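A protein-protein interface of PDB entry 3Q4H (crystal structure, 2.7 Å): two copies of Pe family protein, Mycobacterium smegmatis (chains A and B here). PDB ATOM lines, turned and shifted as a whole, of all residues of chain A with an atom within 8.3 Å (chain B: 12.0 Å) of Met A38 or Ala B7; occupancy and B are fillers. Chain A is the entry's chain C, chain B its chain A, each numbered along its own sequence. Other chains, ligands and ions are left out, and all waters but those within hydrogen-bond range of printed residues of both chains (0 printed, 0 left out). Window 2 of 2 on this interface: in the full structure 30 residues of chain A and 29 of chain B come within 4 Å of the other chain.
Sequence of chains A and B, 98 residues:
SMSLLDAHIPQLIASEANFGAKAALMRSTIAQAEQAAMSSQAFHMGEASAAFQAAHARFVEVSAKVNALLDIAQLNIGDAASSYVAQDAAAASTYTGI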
ATOM      1  N   ALA A  31      13.131   0.464 -15.680  1.00  0.00           N
ATOM      2  CA  ALA A  31      12.498   0.336 -14.380  1.00  0.00           C
ATOM      3  C   ALA A  31      13.297   1.093 -13.334  1.00  0.00           C
ATOM      4  O   ALA A  31      12.730   1.848 -12.540  1.00  0.00           O
ATOM      5  CB  ALA A  31      12.361  -1.130 -13.996  1.00  0.00           C
ATOM      6  N   GLN A  32      14.613   0.904 -13.342  1.00  0.00           N
ATOM      7  CA  GLN A  32      15.493   1.588 -12.399  1.00  0.00           C
ATOM      8  C   GLN A  32      15.421   3.108 -12.546  1.00  0.00           C
ATOM      9  O   GLN A  32      15.310   3.833 -11.559  1.00  0.00           O
ATOM     10  CB  GLN A  32      16.930   1.114 -12.585  1.00  0.00           C
ATOM     11  CG  GLN A  32      17.199  -0.296 -12.035  1.00  0.00           C
ATOM     12  CD  GLN A  32      18.514  -0.877 -12.553  1.00  0.00           C
ATOM     13  OE1 GLN A  32      18.606  -2.079 -12.805  1.00  0.00           O
ATOM     14  NE2 GLN A  32      19.527  -0.019 -12.751  1.00  0.00           N
ATOM     15  N   ALA A  33      15.474   3.572 -13.790  1.00  0.00           N
ATOM     16  CA  ALA A  33      15.321   4.990 -14.118  1.00  0.00           C
ATOM     17  C   ALA A  33      14.009   5.543 -13.566  1.00  0.00           C
ATOM     18  O   ALA A  33      13.963   6.632 -13.001  1.00  0.00           O
ATOM     19  CB  ALA A  33      15.358   5.167 -15.625  1.00  0.00           C
ATOM     20  N   GLU A  34      12.942   4.779 -13.765  1.00  0.00           N
ATOM     21  CA  GLU A  34      11.635   5.086 -13.204  1.00  0.00           C
ATOM     22  C   GLU A  34      11.707   5.240 -11.674  1.00  0.00           C
ATOM     23  O   GLU A  34      11.126   6.174 -11.125  1.00  0.00           O
ATOM     24  CB  GLU A  34      10.626   4.014 -13.648  1.00  0.00           C
ATOM     25  CG  GLU A  34       9.393   3.807 -12.762  1.00  0.00           C
ATOM     26  CD  GLU A  34       8.383   4.919 -12.872  1.00  0.00           C
ATOM     27  OE1 GLU A  34       8.381   5.631 -13.900  1.00  0.00           O
ATOM     28  OE2 GLU A  34       7.585   5.074 -11.920  1.00  0.00           O
ATOM     29  N   GLN A  35      12.436   4.363 -10.988  1.00  0.00           N
ATOM     30  CA  GLN A  35      12.569   4.488  -9.529  1.00  0.00           C
ATOM     31  C   GLN A  35      13.372   5.708  -9.090  1.00  0.00           C
ATOM     32  O   GLN A  35      13.098   6.281  -8.040  1.00  0.00           O
ATOM     33  CB  GLN A  35      13.204   3.249  -8.920  1.00  0.00           C
ATOM     34  CG  GLN A  35      12.362   2.022  -9.025  1.00  0.00           C
ATOM     35  CD  GLN A  35      13.155   0.777  -8.737  1.00  0.00           C
ATOM     36  OE1 GLN A  35      13.680   0.608  -7.639  1.00  0.00           O
ATOM     37  NE2 GLN A  35      13.267  -0.099  -9.730  1.00  0.00           N
ATOM     38  N   ALA A  36      14.379   6.084  -9.869  1.00  0.00           N
ATOM     39  CA  ALA A  36      15.160   7.284  -9.567  1.00  0.00           C
ATOM     40  C   ALA A  36      14.294   8.524  -9.753  1.00  0.00           C
ATOM     41  O   ALA A  36      14.321   9.428  -8.931  1.00  0.00           O
ATOM     42  CB  ALA A  36      16.395   7.358 -10.441  1.00  0.00           C
ATOM     43  N   ALA A  37      13.518   8.547 -10.831  1.00  0.00           N
ATOM     44  CA  ALA A  37      12.569   9.631 -11.094  1.00  0.00           C
ATOM     45  C   ALA A  37      11.492   9.719 -10.018  1.00  0.00           C
ATOM     46  O   ALA A  37      11.114  10.817  -9.614  1.00  0.00           O
ATOM     47  CB  ALA A  37      11.917   9.453 -12.468  1.00  0.00           C
ATOM     48  N   MET A  38      11.005   8.564  -9.566  1.00  0.00           N
ATOM     49  CA  MET A  38       9.993   8.507  -8.514  1.00  0.00           C
ATOM     50  C   MET A  38      10.506   9.100  -7.208  1.00  0.00           C
ATOM     51  O   MET A  38       9.754   9.773  -6.511  1.00  0.00           O
ATOM     52  CB  MET A  38       9.504   7.070  -8.274  1.00  0.00           C
ATOM     53  CG  MET A  38       8.333   6.636  -9.168  1.00  0.00           C
ATOM     54  SD  MET A  38       7.604   4.848  -8.702  1.00  0.00           S
ATOM     55  CE  MET A  38       6.504   5.341  -7.136  1.00  0.00           C
ATOM     56  N   SER A  39      11.772   8.859  -6.871  1.00  0.00           N
ATOM     57  CA  SER A  39      12.328   9.389  -5.616  1.00  0.00           C
ATOM     58  C   SER A  39      12.736  10.863  -5.696  1.00  0.00           C
ATOM     59  O   SER A  39      12.955  11.495  -4.664  1.00  0.00           O
ATOM     60  CB  SER A  39      13.493   8.532  -5.106  1.00  0.00           C
ATOM     61  OG  SER A  39      14.436   8.289  -6.118  1.00  0.00           O
ATOM     62  N   SER A  40      12.804  11.428  -6.900  1.00  0.00           N
ATOM     63  CA  SER A  40      13.043  12.862  -7.031  1.00  0.00           C
ATOM     64  C   SER A  40      11.822  13.654  -6.566  1.00  0.00           C
ATOM     65  O   SER A  40      11.857  14.885  -6.537  1.00  0.00           O
ATOM     66  CB  SER A  40      13.391  13.243  -8.476  1.00  0.00           C
ATOM     67  OG  SER A  40      12.255  13.730  -9.174  1.00  0.00           O
ATOM     68  N   GLN A  41      10.749  12.947  -6.206  1.00  0.00           N
ATOM     69  CA  GLN A  41       9.489  13.586  -5.805  1.00  0.00           C
ATOM     70  C   GLN A  41       9.441  14.120  -4.374  1.00  0.00           C
ATOM     71  O   GLN A  41       8.397  14.585  -3.924  1.00  0.00           O
ATOM     72  CB  GLN A  41       8.290  12.666  -6.078  1.00  0.00           C
ATOM     73  CG  GLN A  41       7.786  12.783  -7.500  1.00  0.00           C
ATOM     74  CD  GLN A  41       7.616  14.238  -7.919  1.00  0.00           C
ATOM     75  OE1 GLN A  41       8.196  14.674  -8.909  1.00  0.00           O
ATOM     76  NE2 GLN A  41       6.858  15.004  -7.137  1.00  0.00           N
ATOM     77  N   ALA A  42      10.563  14.070  -3.668  1.00  0.00           N
ATOM     78  CA  ALA A  42      10.775  14.977  -2.550  1.00  0.00           C
ATOM     79  C   ALA A  42      11.202  16.328  -3.145  1.00  0.00           C
ATOM     80  O   ALA A  42      12.368  16.708  -3.037  1.00  0.00           O
ATOM     81  CB  ALA A  42      11.846  14.426  -1.611  1.00  0.00           C
ATOM     82  N   PHE A  43      10.258  17.035  -3.785  1.00  0.00           N
ATOM     83  CA  PHE A  43      10.574  18.264  -4.535  1.00  0.00           C
ATOM     84  C   PHE A  43       9.386  19.139  -4.997  1.00  0.00           C
ATOM     85  O   PHE A  43       9.201  20.248  -4.490  1.00  0.00           O
ATOM     86  CB  PHE A  43      11.428  17.913  -5.760  1.00  0.00           C
ATOM     87  N   HIS A  44       8.591  18.649  -5.954  1.00  0.00           N
ATOM     88  CA  HIS A  44       7.758  19.531  -6.819  1.00  0.00           C
ATOM     89  C   HIS A  44       6.387  19.930  -6.281  1.00  0.00           C
ATOM     90  O   HIS A  44       5.833  19.265  -5.408  1.00  0.00           O
ATOM     91  CB  HIS A  44       7.536  18.881  -8.197  1.00  0.00           C
ATOM     92  CG  HIS A  44       8.775  18.301  -8.793  1.00  0.00           C
ATOM     93  ND1 HIS A  44       9.098  16.967  -8.678  1.00  0.00           N
ATOM     94  CD2 HIS A  44       9.784  18.877  -9.486  1.00  0.00           C
ATOM     95  CE1 HIS A  44      10.250  16.743  -9.287  1.00  0.00           C
ATOM     96  NE2 HIS A  44      10.687  17.886  -9.784  1.00  0.00           N
ATOM     97  N   PHE A  52       6.020  17.685 -14.382  1.00  0.00           N
ATOM     98  CA  PHE A  52       6.608  16.402 -14.009  1.00  0.00           C
ATOM     99  C   PHE A  52       5.648  15.236 -14.229  1.00  0.00           C
ATOM    100  O   PHE A  52       6.035  14.203 -14.769  1.00  0.00           O
ATOM    101  CB  PHE A  52       7.055  16.414 -12.552  1.00  0.00           C
ATOM    102  CG  PHE A  52       7.824  15.193 -12.163  1.00  0.00           C
ATOM    103  CD1 PHE A  52       7.160  14.037 -11.763  1.00  0.00           C
ATOM    104  CD2 PHE A  52       9.208  15.192 -12.222  1.00  0.00           C
ATOM    105  CE1 PHE A  52       7.862  12.902 -11.419  1.00  0.00           C
ATOM    106  CE2 PHE A  52       9.924  14.068 -11.880  1.00  0.00           C
ATOM    107  CZ  PHE A  52       9.250  12.914 -11.478  1.00  0.00           C
ATOM    108  N   HIS A  56       6.156  12.308 -16.739  1.00  0.00           N
ATOM    109  CA  HIS A  56       6.128  10.932 -16.230  1.00  0.00           C
ATOM    110  C   HIS A  56       5.183  10.056 -17.048  1.00  0.00           C
ATOM    111  O   HIS A  56       5.582   9.016 -17.574  1.00  0.00           O
ATOM    112  CB  HIS A  56       5.708  10.907 -14.763  1.00  0.00           C
ATOM    113  CG  HIS A  56       5.738   9.539 -14.154  1.00  0.00           C
ATOM    114  ND1 HIS A  56       4.614   8.922 -13.649  1.00  0.00           N
ATOM    115  CD2 HIS A  56       6.758   8.664 -13.977  1.00  0.00           C
ATOM    116  CE1 HIS A  56       4.939   7.724 -13.191  1.00  0.00           C
ATOM    117  NE2 HIS A  56       6.232   7.542 -13.378  1.00  0.00           N
ATOM    118  N   VAL A  60       6.158   6.669 -19.022  1.00  0.00           N
ATOM    119  CA  VAL A  60       5.464   5.381 -18.881  1.00  0.00           C
ATOM    120  C   VAL A  60       4.974   4.910 -20.254  1.00  0.00           C
ATOM    121  O   VAL A  60       5.253   3.793 -20.667  1.00  0.00           O
ATOM    122  CB  VAL A  60       4.274   5.462 -17.882  1.00  0.00           C
ATOM    123  CG1 VAL A  60       3.454   4.193 -17.924  1.00  0.00           C
ATOM    124  CG2 VAL A  60       4.786   5.709 -16.472  1.00  0.00           C
ATOM    125  N   ASP B   6       2.767   0.015  -5.387  1.00  0.00           N
ATOM    126  CA  ASP B   6       2.898   1.126  -6.377  1.00  0.00           C
ATOM    127  C   ASP B   6       4.351   1.284  -6.820  1.00  0.00           C
ATOM    128  O   ASP B   6       4.669   1.072  -7.989  1.00  0.00           O
ATOM    129  CB  ASP B   6       2.382   2.439  -5.786  1.00  0.00           C
ATOM    130  N   ALA B   7       5.224   1.656  -5.885  1.00  0.00           N
ATOM    131  CA  ALA B   7       6.675   1.677  -6.128  1.00  0.00           C
ATOM    132  C   ALA B   7       7.241   0.256  -6.121  1.00  0.00           C
ATOM    133  O   ALA B   7       8.381   0.032  -6.531  1.00  0.00           O
ATOM    134  CB  ALA B   7       7.382   2.533  -5.088  1.00  0.00           C
ATOM    135  N   HIS B   8       6.436  -0.689  -5.633  1.00  0.00           N
ATOM    136  CA  HIS B   8       6.711  -2.132  -5.720  1.00  0.00           C
ATOM    137  C   HIS B   8       6.761  -2.636  -7.178  1.00  0.00           C
ATOM    138  O   HIS B   8       7.425  -3.632  -7.469  1.00  0.00           O
ATOM    139  CB  HIS B   8       5.641  -2.878  -4.885  1.00  0.00           C
ATOM    140  CG  HIS B   8       5.498  -4.342  -5.190  1.00  0.00           C
ATOM    141  ND1 HIS B   8       6.144  -5.324  -4.464  1.00  0.00           N
ATOM    142  CD2 HIS B   8       4.732  -4.993  -6.099  1.00  0.00           C
ATOM    143  CE1 HIS B   8       5.805  -6.513  -4.934  1.00  0.00           C
ATOM    144  NE2 HIS B   8       4.950  -6.340  -5.927  1.00  0.00           N
ATOM    145  N   ILE B   9       6.076  -1.942  -8.088  1.00  0.00           N
ATOM    146  CA  ILE B   9       5.971  -2.386  -9.488  1.00  0.00           C
ATOM    147  C   ILE B   9       7.304  -2.261 -10.259  1.00  0.00           C
ATOM    148  O   ILE B   9       7.760  -3.237 -10.863  1.00  0.00           O
ATOM    149  CB  ILE B   9       4.808  -1.659 -10.233  1.00  0.00           C
ATOM    150  CG1 ILE B   9       3.448  -2.109  -9.687  1.00  0.00           C
ATOM    151  CG2 ILE B   9       4.873  -1.910 -11.728  1.00  0.00           C
ATOM    152  CD1 ILE B   9       3.107  -3.570  -9.976  1.00  0.00           C
ATOM    153  N   PRO B  10       7.932  -1.067 -10.242  1.00  0.00           N
ATOM    154  CA  PRO B  10       9.269  -0.945 -10.806  1.00  0.00           C
ATOM    155  C   PRO B  10      10.296  -1.934 -10.247  1.00  0.00           C
ATOM    156  O   PRO B  10      11.166  -2.387 -10.989  1.00  0.00           O
ATOM    157  CB  PRO B  10       9.664   0.477 -10.430  1.00  0.00           C
ATOM    158  CG  PRO B  10       8.409   1.209 -10.394  1.00  0.00           C
ATOM    159  CD  PRO B  10       7.361   0.255  -9.934  1.00  0.00           C
ATOM    160  N   GLN B  11      10.205  -2.253  -8.959  1.00  0.00           N
ATOM    161  CA  GLN B  11      11.112  -3.225  -8.357  1.00  0.00           C
ATOM    162  C   GLN B  11      10.888  -4.610  -8.948  1.00  0.00           C
ATOM    163  O   GLN B  11      11.843  -5.307  -9.283  1.00  0.00           O
ATOM    164  CB  GLN B  11      10.947  -3.249  -6.842  1.00  0.00           C
ATOM    165  CG  GLN B  11      11.410  -1.961  -6.190  1.00  0.00           C
ATOM    166  CD  GLN B  11      11.286  -1.969  -4.675  1.00  0.00           C
ATOM    167  OE1 GLN B  11      10.910  -0.964  -4.065  1.00  0.00           O
ATOM    168  NE2 GLN B  11      11.604  -3.103  -4.057  1.00  0.00           N
ATOM    169  N   LEU B  12       9.623  -4.991  -9.092  1.00  0.00           N
ATOM    170  CA  LEU B  12       9.257  -6.277  -9.677  1.00  0.00           C
ATOM    171  C   LEU B  12       9.744  -6.392 -11.115  1.00  0.00           C
ATOM    172  O   LEU B  12      10.423  -7.358 -11.468  1.00  0.00           O
ATOM    173  CB  LEU B  12       7.743  -6.463  -9.629  1.00  0.00           C
ATOM    174  CG  LEU B  12       7.169  -7.792 -10.127  1.00  0.00           C
ATOM    175  CD1 LEU B  12       7.749  -8.995  -9.360  1.00  0.00           C
ATOM    176  CD2 LEU B  12       5.635  -7.776 -10.040  1.00  0.00           C
ATOM    177  N   ILE B  13       9.383  -5.404 -11.935  1.00  0.00           N
ATOM    178  CA  ILE B  13       9.812  -5.314 -13.332  1.00  0.00           C
ATOM    179  C   ILE B  13      11.324  -5.437 -13.435  1.00  0.00           C
ATOM    180  O   ILE B  13      11.833  -6.165 -14.283  1.00  0.00           O
ATOM    181  CB  ILE B  13       9.408  -3.960 -13.957  1.00  0.00           C
ATOM    182  CG1 ILE B  13       7.892  -3.872 -14.136  1.00  0.00           C
ATOM    183  CG2 ILE B  13      10.113  -3.733 -15.301  1.00  0.00           C
ATOM    184  CD1 ILE B  13       7.400  -2.468 -14.366  1.00  0.00           C
ATOM    185  N   ALA B  14      12.034  -4.716 -12.573  1.00  0.00           N
ATOM    186  CA  ALA B  14      13.484  -4.744 -12.575  1.00  0.00           C
ATOM    187  C   ALA B  14      13.946  -6.150 -12.215  1.00  0.00           C
ATOM    188  O   ALA B  14      14.710  -6.759 -12.954  1.00  0.00           O
ATOM    189  CB  ALA B  14      14.046  -3.716 -11.609  1.00  0.00           C
ATOM    190  N   SER B  15      13.445  -6.682 -11.103  1.00  0.00           N
ATOM    191  CA  SER B  15      13.841  -8.018 -10.649  1.00  0.00           C
ATOM    192  C   SER B  15      13.649  -9.075 -11.725  1.00  0.00           C
ATOM    193  O   SER B  15      14.476  -9.959 -11.883  1.00  0.00           O
ATOM    194  CB  SER B  15      13.057  -8.426  -9.398  1.00  0.00           C
ATOM    195  OG  SER B  15      13.502  -7.709  -8.261  1.00  0.00           O
ATOM    196  N   GLU B  16      12.547  -8.980 -12.458  1.00  0.00           N
ATOM    197  CA  GLU B  16      12.223  -9.976 -13.456  1.00  0.00           C
ATOM    198  C   GLU B  16      13.088  -9.788 -14.690  1.00  0.00           C
ATOM    199  O   GLU B  16      13.577 -10.771 -15.257  1.00  0.00           O
ATOM    200  CB  GLU B  16      10.735  -9.923 -13.804  1.00  0.00           C
ATOM    201  CG  GLU B  16       9.840 -10.488 -12.692  1.00  0.00           C
ATOM    202  CD  GLU B  16       8.356 -10.397 -12.998  1.00  0.00           C
ATOM    203  OE1 GLU B  16       7.975  -9.728 -13.976  1.00  0.00           O
ATOM    204  OE2 GLU B  16       7.565 -10.993 -12.249  1.00  0.00           O
ATOM    205  N   VAL B  85       4.087  -6.883 -17.057  1.00  0.00           N
ATOM    206  CA  VAL B  85       3.882  -5.972 -15.929  1.00  0.00           C
ATOM    207  C   VAL B  85       4.092  -4.520 -16.333  1.00  0.00           C
ATOM    208  O   VAL B  85       3.351  -3.642 -15.894  1.00  0.00           O
ATOM    209  CB  VAL B  85       4.827  -6.272 -14.753  1.00  0.00           C
ATOM    210  CG1 VAL B  85       4.697  -5.179 -13.680  1.00  0.00           C
ATOM    211  CG2 VAL B  85       4.541  -7.651 -14.174  1.00  0.00           C
ATOM    212  N   ALA B  86       5.112  -4.279 -17.159  1.00  0.00           N
ATOM    213  CA  ALA B  86       5.424  -2.933 -17.652  1.00  0.00           C
ATOM    214  C   ALA B  86       4.305  -2.395 -18.540  1.00  0.00           C
ATOM    215  O   ALA B  86       3.828  -1.273 -18.346  1.00  0.00           O
ATOM    216  CB  ALA B  86       6.740  -2.939 -18.423  1.00  0.00           C
ATOM    217  N   ALA B  89       1.058  -2.012 -16.541  1.00  0.00           N
ATOM    218  CA  ALA B  89       1.145  -0.806 -15.710  1.00  0.00           C
ATOM    219  C   ALA B  89       0.843   0.465 -16.512  1.00  0.00           C
ATOM    220  O   ALA B  89       0.265   1.412 -15.980  1.00  0.00           O
ATOM    221  CB  ALA B  89       2.510  -0.704 -15.065  1.00  0.00           C
ATOM    222  N   ALA B  90       1.226   0.474 -17.789  1.00  0.00           N
ATOM    223  CA  ALA B  90       1.019   1.638 -18.661  1.00  0.00           C
ATOM    224  C   ALA B  90      -0.440   1.806 -19.086  1.00  0.00           C
ATOM    225  O   ALA B  90      -0.933   2.930 -19.182  1.00  0.00           O
ATOM    226  CB  ALA B  90       1.913   1.535 -19.894  1.00  0.00           C
ATOM    227  N   SER B  93      -2.361   2.969 -16.086  1.00  0.00           N
ATOM    228  CA  SER B  93      -1.944   4.317 -15.684  1.00  0.00           C
ATOM    229  C   SER B  93      -2.653   5.410 -16.470  1.00  0.00           C
ATOM    230  O   SER B  93      -3.106   6.402 -15.890  1.00  0.00           O
ATOM    231  CB  SER B  93      -0.427   4.481 -15.848  1.00  0.00           C
ATOM    232  OG  SER B  93       0.282   3.488 -15.117  1.00  0.00           O
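The backbone carbonyl oxygen (O) of Pro B10 is in hydrogen-bond range of the side-chain amide nitrogen (NE2) of Gln A35 (3.4 Å).
OG of Ser B15 is in hydrogen-bond range of O of Gln B11, 3.1 Å away.
O of Ala A31 sits at hydrogen-bond distance from NE2 of Gln A35 (3.5 Å).
OE1 of Glu A34 lies within hydrogen-bond range of NE2 of His A56, 2.9 Å away.
The side-chain hydroxyl of Ser A39 lies within hydrogen-bond range of the backbone carbonyl oxygen of Gln A35, at 3.1 Å.
Among the printed residues, merely in contact across the chains: Ala A31 with Pro B10 (3.5 Å), Ala A31 with Ile B13 (3.7 Å), Ala A31 with Ala B14 (3.9 Å), Glu A34 with Pro B10 (3.7 Å), Gln A35 with Gln B11 (3.7 Å), Met A38 with Ala B7 (3.6 Å) and Val A60 with Ala B90 (3.6 Å).
Of chain B, only Pro B10 comes within 4 Å of Glu A34.
Of chain B, only Pro B10 (3.4 Å) and Gln B11 (3.7 Å) come within 4 Å of Gln A35.
No residue of chain B comes within 4 Å of Ala A36.
Ala A37 touches none of the printed residues of chain B.
No residue of chain B comes within 4 Å of Ser A39.
Of the printed residues of chain A, Ala B7 touches Met A38.
Of the printed residues of chain A, Gln B11 touches Gln A35.
Printed residues of chain A within 4 Å of Ile B13: Ala A31.
Of the printed residues of chain A, Ala B14 touches Ala A31.
The nearest residue of chain B that does not touch Met A38 is Pro B10 (4.1 Å).
The nearest residue of chain A that does not touch Ala B7 is Gln A35 (5.1 Å).
Printed residues of chain A that touch a printed residue of chain B: Ala A31, Glu A34, Gln A35, Met A38 and Val A60.
Hydrophobic or aromatic side chains of chain A that line the printed part of chain B: Ala A31, Met A38 and Val A60.
Of the 16 printed residues of chain B, 6 touch a printed residue of chain A.
Hydrophobic or aromatic side chains of chain B within 4 Å of the printed part of chain A: Ala B7, Pro B10, Ile B13, Ala B14 and Ala B90.
Among the printed residues, 8 pairs touch across the chains.
Among the printed residues, no Asp or Glu carboxylate lies within 4 Å of a Lys or Arg side-chain nitrogen of the other chain.
No position is printed for both chains.
Of the 8 pairs that touch across the chains among the printed residues, none has its exchanged pair printed and touching as well.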
